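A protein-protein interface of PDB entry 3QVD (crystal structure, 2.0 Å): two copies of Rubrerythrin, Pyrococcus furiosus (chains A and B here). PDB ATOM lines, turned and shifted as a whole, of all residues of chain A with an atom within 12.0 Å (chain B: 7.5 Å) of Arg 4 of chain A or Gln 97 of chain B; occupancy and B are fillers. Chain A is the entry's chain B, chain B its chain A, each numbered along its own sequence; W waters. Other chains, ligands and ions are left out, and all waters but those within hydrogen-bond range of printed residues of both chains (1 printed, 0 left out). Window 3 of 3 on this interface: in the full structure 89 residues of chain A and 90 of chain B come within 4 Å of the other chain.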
ATOM      1  N   VAL A   1     -20.455  13.824 -21.471  1.00  0.00           N
ATOM      2  CA  VAL A   1     -20.056  13.207 -22.769  1.00  0.00           C
ATOM      3  C   VAL A   1     -19.099  12.043 -22.518  1.00  0.00           C
ATOM      4  O   VAL A   1     -18.182  12.154 -21.706  1.00  0.00           O
ATOM      5  CB  VAL A   1     -19.355  14.243 -23.685  1.00  0.00           C
ATOM      6  CG1 VAL A   1     -18.995  13.604 -25.023  1.00  0.00           C
ATOM      7  CG2 VAL A   1     -20.264  15.450 -23.900  1.00  0.00           C
ATOM      8  N   VAL A   2     -19.328  10.931 -23.214  1.00  0.00           N
ATOM      9  CA  VAL A   2     -18.494   9.735 -23.095  1.00  0.00           C
ATOM     10  C   VAL A   2     -17.096  10.018 -23.651  1.00  0.00           C
ATOM     11  O   VAL A   2     -16.962  10.609 -24.723  1.00  0.00           O
ATOM     12  CB  VAL A   2     -19.142   8.552 -23.861  1.00  0.00           C
ATOM     13  CG1 VAL A   2     -18.204   7.351 -23.892  1.00  0.00           C
ATOM     14  CG2 VAL A   2     -20.463   8.176 -23.193  1.00  0.00           C
ATOM     15  N   LYS A   3     -16.062   9.578 -22.934  1.00  0.00           N
ATOM     16  CA  LYS A   3     -14.678   9.824 -23.339  1.00  0.00           C
ATOM     17  C   LYS A   3     -13.796   8.589 -23.573  1.00  0.00           C
ATOM     18  O   LYS A   3     -12.919   8.610 -24.434  1.00  0.00           O
ATOM     19  CB  LYS A   3     -13.996  10.713 -22.296  1.00  0.00           C
ATOM     20  CG  LYS A   3     -14.653  12.075 -22.073  1.00  0.00           C
ATOM     21  CD  LYS A   3     -14.370  13.023 -23.223  1.00  0.00           C
ATOM     22  CE  LYS A   3     -14.779  14.451 -22.875  1.00  0.00           C
ATOM     23  NZ  LYS A   3     -14.492  15.396 -23.990  1.00  0.00           N
ATOM     24  N   ARG A   4     -14.003   7.529 -22.798  1.00  0.00           N
ATOM     25  CA  ARG A   4     -13.189   6.319 -22.946  1.00  0.00           C
ATOM     26  C   ARG A   4     -13.264   5.785 -24.376  1.00  0.00           C
ATOM     27  O   ARG A   4     -14.334   5.728 -24.985  1.00  0.00           O
ATOM     28  CB  ARG A   4     -13.634   5.257 -21.935  1.00  0.00           C
ATOM     29  CG  ARG A   4     -13.509   5.713 -20.478  1.00  0.00           C
ATOM     30  CD  ARG A   4     -12.053   5.887 -20.058  1.00  0.00           C
ATOM     31  NE  ARG A   4     -11.394   4.611 -19.784  1.00  0.00           N
ATOM     32  CZ  ARG A   4     -11.461   3.966 -18.620  1.00  0.00           C
ATOM     33  NH1 ARG A   4     -10.835   2.807 -18.465  1.00  0.00           N
ATOM     34  NH2 ARG A   4     -12.133   4.486 -17.602  1.00  0.00           N
ATOM     35  N   THR A   5     -12.111   5.401 -24.911  1.00  0.00           N
ATOM     36  CA  THR A   5     -12.022   4.917 -26.281  1.00  0.00           C
ATOM     37  C   THR A   5     -12.927   3.740 -26.644  1.00  0.00           C
ATOM     38  O   THR A   5     -13.660   3.811 -27.632  1.00  0.00           O
ATOM     39  CB  THR A   5     -10.565   4.557 -26.646  1.00  0.00           C
ATOM     40  OG1 THR A   5      -9.720   5.691 -26.402  1.00  0.00           O
ATOM     41  CG2 THR A   5     -10.460   4.192 -28.124  1.00  0.00           C
ATOM     42  N   MET A   6     -12.895   2.667 -25.860  1.00  0.00           N
ATOM     43  CA  MET A   6     -13.727   1.510 -26.189  1.00  0.00           C
ATOM     44  C   MET A   6     -15.227   1.797 -26.117  1.00  0.00           C
ATOM     45  O   MET A   6     -15.972   1.434 -27.023  1.00  0.00           O
ATOM     46  CB  MET A   6     -13.377   0.317 -25.291  1.00  0.00           C
ATOM     47  CG  MET A   6     -11.944  -0.195 -25.460  1.00  0.00           C
ATOM     48  SD  MET A   6     -11.431  -0.439 -27.193  1.00  0.00           S
ATOM     49  CE  MET A   6     -12.462  -1.834 -27.682  1.00  0.00           C
ATOM     50  N   THR A   7     -15.668   2.453 -25.049  1.00  0.00           N
ATOM     51  CA  THR A   7     -17.084   2.764 -24.894  1.00  0.00           C
ATOM     52  C   THR A   7     -17.556   3.705 -25.995  1.00  0.00           C
ATOM     53  O   THR A   7     -18.670   3.573 -26.506  1.00  0.00           O
ATOM     54  CB  THR A   7     -17.374   3.382 -23.508  1.00  0.00           C
ATOM     55  OG1 THR A   7     -17.129   2.397 -22.495  1.00  0.00           O
ATOM     56  CG2 THR A   7     -18.837   3.852 -23.416  1.00  0.00           C
ATOM     57  N   LYS A   8     -16.700   4.648 -26.374  1.00  0.00           N
ATOM     58  CA  LYS A   8     -17.037   5.580 -27.435  1.00  0.00           C
ATOM     59  C   LYS A   8     -17.241   4.810 -28.740  1.00  0.00           C
ATOM     60  O   LYS A   8     -18.198   5.060 -29.478  1.00  0.00           O
ATOM     61  CB  LYS A   8     -15.923   6.613 -27.593  1.00  0.00           C
ATOM     62  CG  LYS A   8     -16.131   7.587 -28.732  1.00  0.00           C
ATOM     63  CD  LYS A   8     -15.252   8.824 -28.565  1.00  0.00           C
ATOM     64  CE  LYS A   8     -13.781   8.467 -28.489  1.00  0.00           C
ATOM     65  NZ  LYS A   8     -12.940   9.683 -28.306  1.00  0.00           N
ATOM     66  N   LYS A   9     -16.337   3.875 -29.016  1.00  0.00           N
ATOM     67  CA  LYS A   9     -16.412   3.043 -30.218  1.00  0.00           C
ATOM     68  C   LYS A   9     -17.701   2.223 -30.218  1.00  0.00           C
ATOM     69  O   LYS A   9     -18.382   2.123 -31.240  1.00  0.00           O
ATOM     70  CB  LYS A   9     -15.200   2.101 -30.285  1.00  0.00           C
ATOM     71  CG  LYS A   9     -15.173   1.169 -31.491  1.00  0.00           C
ATOM     72  CD  LYS A   9     -13.806   0.491 -31.612  1.00  0.00           C
ATOM     73  CE  LYS A   9     -13.742  -0.465 -32.798  1.00  0.00           C
ATOM     74  NZ  LYS A   9     -14.635  -1.638 -32.606  1.00  0.00           N
ATOM     75  N   PHE A  10     -18.027   1.635 -29.072  1.00  0.00           N
ATOM     76  CA  PHE A  10     -19.237   0.830 -28.948  1.00  0.00           C
ATOM     77  C   PHE A  10     -20.489   1.681 -29.179  1.00  0.00           C
ATOM     78  O   PHE A  10     -21.437   1.228 -29.826  1.00  0.00           O
ATOM     79  CB  PHE A  10     -19.290   0.152 -27.570  1.00  0.00           C
ATOM     80  CG  PHE A  10     -18.230  -0.907 -27.365  1.00  0.00           C
ATOM     81  CD1 PHE A  10     -17.935  -1.377 -26.085  1.00  0.00           C
ATOM     82  CD2 PHE A  10     -17.527  -1.434 -28.448  1.00  0.00           C
ATOM     83  CE1 PHE A  10     -16.951  -2.354 -25.884  1.00  0.00           C
ATOM     84  CE2 PHE A  10     -16.541  -2.413 -28.260  1.00  0.00           C
ATOM     85  CZ  PHE A  10     -16.253  -2.871 -26.976  1.00  0.00           C
ATOM     86  N   LEU A  11     -20.504   2.911 -28.663  1.00  0.00           N
ATOM     87  CA  LEU A  11     -21.667   3.774 -28.868  1.00  0.00           C
ATOM     88  C   LEU A  11     -21.776   4.197 -30.320  1.00  0.00           C
ATOM     89  O   LEU A  11     -22.877   4.392 -30.825  1.00  0.00           O
ATOM     90  CB  LEU A  11     -21.621   5.024 -27.978  1.00  0.00           C
ATOM     91  CG  LEU A  11     -21.946   4.842 -26.494  1.00  0.00           C
ATOM     92  CD1 LEU A  11     -22.158   6.218 -25.853  1.00  0.00           C
ATOM     93  CD2 LEU A  11     -23.201   3.997 -26.335  1.00  0.00           C
ATOM     94  N   GLU A  12     -20.641   4.357 -30.995  1.00  0.00           N
ATOM     95  CA  GLU A  12     -20.684   4.727 -32.406  1.00  0.00           C
ATOM     96  C   GLU A  12     -21.236   3.521 -33.162  1.00  0.00           C
ATOM     97  O   GLU A  12     -22.047   3.665 -34.072  1.00  0.00           O
ATOM     98  CB  GLU A  12     -19.286   5.109 -32.910  1.00  0.00           C
ATOM     99  CG  GLU A  12     -18.704   6.317 -32.162  1.00  0.00           C
ATOM    100  CD  GLU A  12     -17.251   6.606 -32.505  1.00  0.00           C
ATOM    101  OE1 GLU A  12     -16.458   5.645 -32.620  1.00  0.00           O
ATOM    102  OE2 GLU A  12     -16.897   7.797 -32.640  1.00  0.00           O
ATOM    103  N   GLU A  13     -20.812   2.324 -32.765  1.00  0.00           N
ATOM    104  CA  GLU A  13     -21.310   1.100 -33.392  1.00  0.00           C
ATOM    105  C   GLU A  13     -22.807   0.926 -33.128  1.00  0.00           C
ATOM    106  O   GLU A  13     -23.565   0.526 -34.024  1.00  0.00           O
ATOM    107  CB  GLU A  13     -20.539  -0.113 -32.868  1.00  0.00           C
ATOM    108  CG  GLU A  13     -19.108  -0.173 -33.374  1.00  0.00           C
ATOM    109  CD  GLU A  13     -18.322  -1.346 -32.809  1.00  0.00           C
ATOM    110  OE1 GLU A  13     -18.797  -2.495 -32.923  1.00  0.00           O
ATOM    111  OE2 GLU A  13     -17.226  -1.116 -32.260  1.00  0.00           O
ATOM    112  N   HIS A  58     -27.676   7.688 -27.904  1.00  0.00           N
ATOM    113  CA  HIS A  58     -26.245   7.411 -28.065  1.00  0.00           C
ATOM    114  C   HIS A  58     -25.533   8.623 -28.667  1.00  0.00           C
ATOM    115  O   HIS A  58     -24.453   9.009 -28.214  1.00  0.00           O
ATOM    116  CB  HIS A  58     -26.003   6.204 -28.982  1.00  0.00           C
ATOM    117  CG  HIS A  58     -26.657   4.938 -28.517  1.00  0.00           C
ATOM    118  ND1 HIS A  58     -26.713   4.568 -27.191  1.00  0.00           N
ATOM    119  CD2 HIS A  58     -27.249   3.937 -29.210  1.00  0.00           C
ATOM    120  CE1 HIS A  58     -27.310   3.394 -27.087  1.00  0.00           C
ATOM    121  NE2 HIS A  58     -27.645   2.989 -28.298  1.00  0.00           N
ATOM    122  N   ALA A  61     -25.082  11.180 -26.141  1.00  0.00           N
ATOM    123  CA  ALA A  61     -24.110  10.701 -25.160  1.00  0.00           C
ATOM    124  C   ALA A  61     -22.705  10.898 -25.705  1.00  0.00           C
ATOM    125  O   ALA A  61     -21.766  11.147 -24.949  1.00  0.00           O
ATOM    126  CB  ALA A  61     -24.345   9.224 -24.853  1.00  0.00           C
ATOM    127  N   LEU A  62     -22.575  10.776 -27.025  1.00  0.00           N
ATOM    128  CA  LEU A  62     -21.301  10.953 -27.711  1.00  0.00           C
ATOM    129  C   LEU A  62     -20.993  12.441 -27.886  1.00  0.00           C
ATOM    130  O   LEU A  62     -19.897  12.810 -28.314  1.00  0.00           O
ATOM    131  CB  LEU A  62     -21.346  10.277 -29.079  1.00  0.00           C
ATOM    132  CG  LEU A  62     -21.358   8.746 -29.054  1.00  0.00           C
ATOM    133  CD1 LEU A  62     -21.703   8.217 -30.437  1.00  0.00           C
ATOM    134  CD2 LEU A  62     -19.994   8.235 -28.593  1.00  0.00           C
ATOM    135  N   GLY A  63     -21.975  13.279 -27.564  1.00  0.00           N
ATOM    136  CA  GLY A  63     -21.813  14.723 -27.664  1.00  0.00           C
ATOM    137  C   GLY A  63     -21.784  15.282 -29.075  1.00  0.00           C
ATOM    138  O   GLY A  63     -21.172  16.323 -29.317  1.00  0.00           O
ATOM    139  N   LYS A  64     -22.459  14.619 -30.008  1.00  0.00           N
ATOM    140  CA  LYS A  64     -22.450  15.080 -31.391  1.00  0.00           C
ATOM    141  C   LYS A  64     -23.586  16.014 -31.806  1.00  0.00           C
ATOM    142  O   LYS A  64     -23.649  16.441 -32.960  1.00  0.00           O
ATOM    143  CB  LYS A  64     -22.390  13.874 -32.336  1.00  0.00           C
ATOM    144  CG  LYS A  64     -21.054  13.147 -32.296  1.00  0.00           C
ATOM    145  CD  LYS A  64     -20.881  12.231 -33.500  1.00  0.00           C
ATOM    146  CE  LYS A  64     -19.514  11.564 -33.504  1.00  0.00           C
ATOM    147  NZ  LYS A  64     -19.329  10.662 -32.329  1.00  0.00           N
ATOM    148  N   ASN B  91     -23.066  -2.710 -22.490  1.00  0.00           N
ATOM    149  CA  ASN B  91     -23.474  -2.189 -21.191  1.00  0.00           C
ATOM    150  C   ASN B  91     -22.432  -2.556 -20.132  1.00  0.00           C
ATOM    151  O   ASN B  91     -22.010  -1.708 -19.339  1.00  0.00           O
ATOM    152  CB  ASN B  91     -24.854  -2.755 -20.829  1.00  0.00           C
ATOM    153  CG  ASN B  91     -25.307  -2.372 -19.432  1.00  0.00           C
ATOM    154  OD1 ASN B  91     -25.134  -3.138 -18.486  1.00  0.00           O
ATOM    155  ND2 ASN B  91     -25.893  -1.179 -19.295  1.00  0.00           N
ATOM    156  N   LYS B  92     -22.003  -3.818 -20.133  1.00  0.00           N
ATOM    157  CA  LYS B  92     -21.014  -4.278 -19.168  1.00  0.00           C
ATOM    158  C   LYS B  92     -19.695  -3.535 -19.360  1.00  0.00           C
ATOM    159  O   LYS B  92     -18.994  -3.232 -18.391  1.00  0.00           O
ATOM    160  CB  LYS B  92     -20.777  -5.779 -19.329  1.00  0.00           C
ATOM    161  CG  LYS B  92     -19.957  -6.397 -18.205  1.00  0.00           C
ATOM    162  CD  LYS B  92     -20.688  -6.238 -16.877  1.00  0.00           C
ATOM    163  CE  LYS B  92     -19.988  -6.960 -15.744  1.00  0.00           C
ATOM    164  NZ  LYS B  92     -20.701  -6.734 -14.450  1.00  0.00           N
ATOM    165  N   ALA B  93     -19.357  -3.251 -20.615  1.00  0.00           N
ATOM    166  CA  ALA B  93     -18.121  -2.542 -20.921  1.00  0.00           C
ATOM    167  C   ALA B  93     -18.197  -1.108 -20.392  1.00  0.00           C
ATOM    168  O   ALA B  93     -17.260  -0.630 -19.755  1.00  0.00           O
ATOM    169  CB  ALA B  93     -17.869  -2.542 -22.433  1.00  0.00           C
ATOM    170  N   ALA B  94     -19.311  -0.428 -20.656  1.00  0.00           N
ATOM    171  CA  ALA B  94     -19.478   0.947 -20.181  1.00  0.00           C
ATOM    172  C   ALA B  94     -19.390   0.957 -18.658  1.00  0.00           C
ATOM    173  O   ALA B  94     -18.769   1.841 -18.064  1.00  0.00           O
ATOM    174  CB  ALA B  94     -20.825   1.506 -20.639  1.00  0.00           C
ATOM    175  N   GLU B  95     -20.011  -0.031 -18.027  1.00  0.00           N
ATOM    176  CA  GLU B  95     -19.980  -0.133 -16.574  1.00  0.00           C
ATOM    177  C   GLU B  95     -18.525  -0.259 -16.143  1.00  0.00           C
ATOM    178  O   GLU B  95     -18.058   0.471 -15.266  1.00  0.00           O
ATOM    179  CB  GLU B  95     -20.762  -1.363 -16.118  1.00  0.00           C
ATOM    180  CG  GLU B  95     -20.588  -1.716 -14.650  1.00  0.00           C
ATOM    181  CD  GLU B  95     -21.219  -3.053 -14.307  1.00  0.00           C
ATOM    182  OE1 GLU B  95     -22.460  -3.174 -14.418  1.00  0.00           O
ATOM    183  OE2 GLU B  95     -20.476  -3.987 -13.936  1.00  0.00           O
ATOM    184  N   PHE B  96     -17.814  -1.180 -16.789  1.00  0.00           N
ATOM    185  CA  PHE B  96     -16.406  -1.442 -16.511  1.00  0.00           C
ATOM    186  C   PHE B  96     -15.518  -0.206 -16.676  1.00  0.00           C
ATOM    187  O   PHE B  96     -14.545  -0.039 -15.948  1.00  0.00           O
ATOM    188  CB  PHE B  96     -15.915  -2.568 -17.432  1.00  0.00           C
ATOM    189  CG  PHE B  96     -14.483  -2.975 -17.205  1.00  0.00           C
ATOM    190  CD1 PHE B  96     -13.510  -2.700 -18.162  1.00  0.00           C
ATOM    191  CD2 PHE B  96     -14.115  -3.668 -16.055  1.00  0.00           C
ATOM    192  CE1 PHE B  96     -12.192  -3.110 -17.984  1.00  0.00           C
ATOM    193  CE2 PHE B  96     -12.791  -4.086 -15.862  1.00  0.00           C
ATOM    194  CZ  PHE B  96     -11.829  -3.807 -16.830  1.00  0.00           C
ATOM    195  N   GLN B  97     -15.840   0.654 -17.638  1.00  0.00           N
ATOM    196  CA  GLN B  97     -15.036   1.856 -17.862  1.00  0.00           C
ATOM    197  C   GLN B  97     -15.601   3.087 -17.159  1.00  0.00           C
ATOM    198  O   GLN B  97     -15.152   4.207 -17.408  1.00  0.00           O
ATOM    199  CB  GLN B  97     -14.895   2.148 -19.363  1.00  0.00           C
ATOM    200  CG  GLN B  97     -14.202   1.045 -20.157  1.00  0.00           C
ATOM    201  CD  GLN B  97     -13.719   1.516 -21.514  1.00  0.00           C
ATOM    202  OE1 GLN B  97     -14.500   1.983 -22.341  1.00  0.00           O
ATOM    203  NE2 GLN B  97     -12.420   1.392 -21.748  1.00  0.00           N
ATOM    204  N   GLY B  98     -16.591   2.875 -16.294  1.00  0.00           N
ATOM    205  CA  GLY B  98     -17.193   3.969 -15.546  1.00  0.00           C
ATOM    206  C   GLY B  98     -17.953   5.040 -16.316  1.00  0.00           C
ATOM    207  O   GLY B  98     -18.128   6.144 -15.809  1.00  0.00           O
ATOM    208  N   GLU B  99     -18.409   4.728 -17.526  1.00  0.00           N
ATOM    209  CA  GLU B  99     -19.152   5.697 -18.338  1.00  0.00           C
ATOM    210  C   GLU B  99     -20.643   5.555 -18.045  1.00  0.00           C
ATOM    211  O   GLU B  99     -21.358   4.827 -18.738  1.00  0.00           O
ATOM    212  CB  GLU B  99     -18.887   5.453 -19.829  1.00  0.00           C
ATOM    213  CG  GLU B  99     -17.461   5.760 -20.281  1.00  0.00           C
ATOM    214  CD  GLU B  99     -17.167   7.255 -20.349  1.00  0.00           C
ATOM    215  OE1 GLU B  99     -16.042   7.621 -20.735  1.00  0.00           O
ATOM    216  OE2 GLU B  99     -18.060   8.066 -20.022  1.00  0.00           O
ATOM    217  N   LYS B 100     -21.102   6.254 -17.010  1.00  0.00           N
ATOM    218  CA  LYS B 100     -22.496   6.191 -16.582  1.00  0.00           C
ATOM    219  C   LYS B 100     -23.491   6.523 -17.684  1.00  0.00           C
ATOM    220  O   LYS B 100     -24.552   5.908 -17.770  1.00  0.00           O
ATOM    221  CB  LYS B 100     -22.729   7.135 -15.395  1.00  0.00           C
ATOM    222  CG  LYS B 100     -21.656   7.065 -14.320  1.00  0.00           C
ATOM    223  CD  LYS B 100     -21.486   5.656 -13.783  1.00  0.00           C
ATOM    224  CE  LYS B 100     -20.356   5.602 -12.765  1.00  0.00           C
ATOM    225  NZ  LYS B 100     -20.163   4.228 -12.220  1.00  0.00           N
ATOM    226  N   VAL B 103     -23.805   3.625 -19.849  1.00  0.00           N
ATOM    227  CA  VAL B 103     -24.464   2.565 -19.101  1.00  0.00           C
ATOM    228  C   VAL B 103     -25.976   2.781 -19.229  1.00  0.00           C
ATOM    229  O   VAL B 103     -26.737   1.830 -19.427  1.00  0.00           O
ATOM    230  CB  VAL B 103     -24.059   2.590 -17.605  1.00  0.00           C
ATOM    231  CG1 VAL B 103     -25.039   1.750 -16.773  1.00  0.00           C
ATOM    232  CG2 VAL B 103     -22.644   2.032 -17.442  1.00  0.00           C
HETATM  233  O   HOH W   1     -10.683  -0.133 -20.296  1.00  0.00           O
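The backbone carbonyl oxygen of Ala 61 of chain A sits at hydrogen-bond distance from the backbone NH of Val 2 of chain A, at 3.0 Å. N of Glu 99 of chain B is in hydrogen-bond range of O of Ala 94 of chain B, at 3.0 Å.
Water W1 bridges the side-chain amide nitrogen of Gln 97 of chain B (2.7 Å) and the guanidinium group of Arg 4 of chain A (3.5 Å).
The guanidinium group (NH2) of Arg 4 of chain A sits at hydrogen-bond distance from the backbone carbonyl oxygen (O) of Gln 97 of chain B (3.0 Å). OE1 of Gln 97 of chain B is in hydrogen-bond range of OG1 of Thr 7 of chain A, 2.7 Å away. The side-chain carboxylate of Glu 99 of chain B lies within hydrogen-bond range of the backbone NH of Arg 4 of chain A (2.9 Å). OE1 of Glu 99 of chain B lies within hydrogen-bond range of N of Lys 3 of chain A (2.9 Å).
Val 2 of chain A touches Glu 99 of chain B. Met 6 of chain A touches Gln 97 of chain B. Thr 7 of chain A touches Ala 94 of chain B (OG1 to CA, 3.6 Å). Thr 7 of chain A touches Glu 99 of chain B (CG2 to CG, 3.9 Å). CE1 of Phe 10 of chain A touches CB of Ala 93 of chain B, at 3.6 Å.
Printed residues of chain A that touch a printed residue of chain B: Val 2, Lys 3, Arg 4, Met 6, Thr 7 and Phe 10. Hydrophobic or aromatic side chains of chain A within 4 Å of the printed part of chain B: Val 2, Met 6 and Phe 10. Among the printed residues, 9 pairs touch across the chains. Among the printed residues, no Asp or Glu carboxylate lies within 4 Å of a Lys or Arg side-chain nitrogen of the other chain.
No position is printed for both chains.
Arg 4 of chain A touches two residues of chain B. Gln 97 of chain B touches just these residues of chain A: Arg 4 (3.0 Å), Met 6 (3.6 Å) and Thr 7 (2.7 Å). Of the printed residues of chain A, Ala 94 of chain B touches Thr 7. No residue of chain A comes within 4 Å of Gly 98 of chain B. Of chain A, only Val 2 (3.5 Å), Lys 3 (2.9 Å), Arg 4 (2.9 Å) and Thr 7 (3.9 Å) come within 4 Å of Glu 99 of chain B. Of the printed residues of chain B, Met 6 of chain A touches Gln 97. Printed residues of chain B within 4 Å of Phe 10 of chain A: Ala 93 (3.6 Å). Printed residues of chain B within 4 Å of Lys 3 of chain A: Glu 99 (2.9 Å). The nearest residue of chain B that does not touch Arg 4 of chain A is Gly 98 of chain B (4.9 Å). The nearest residue of chain A that does not touch Gln 97 of chain B is Thr 5 of chain A (4.9 Å).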
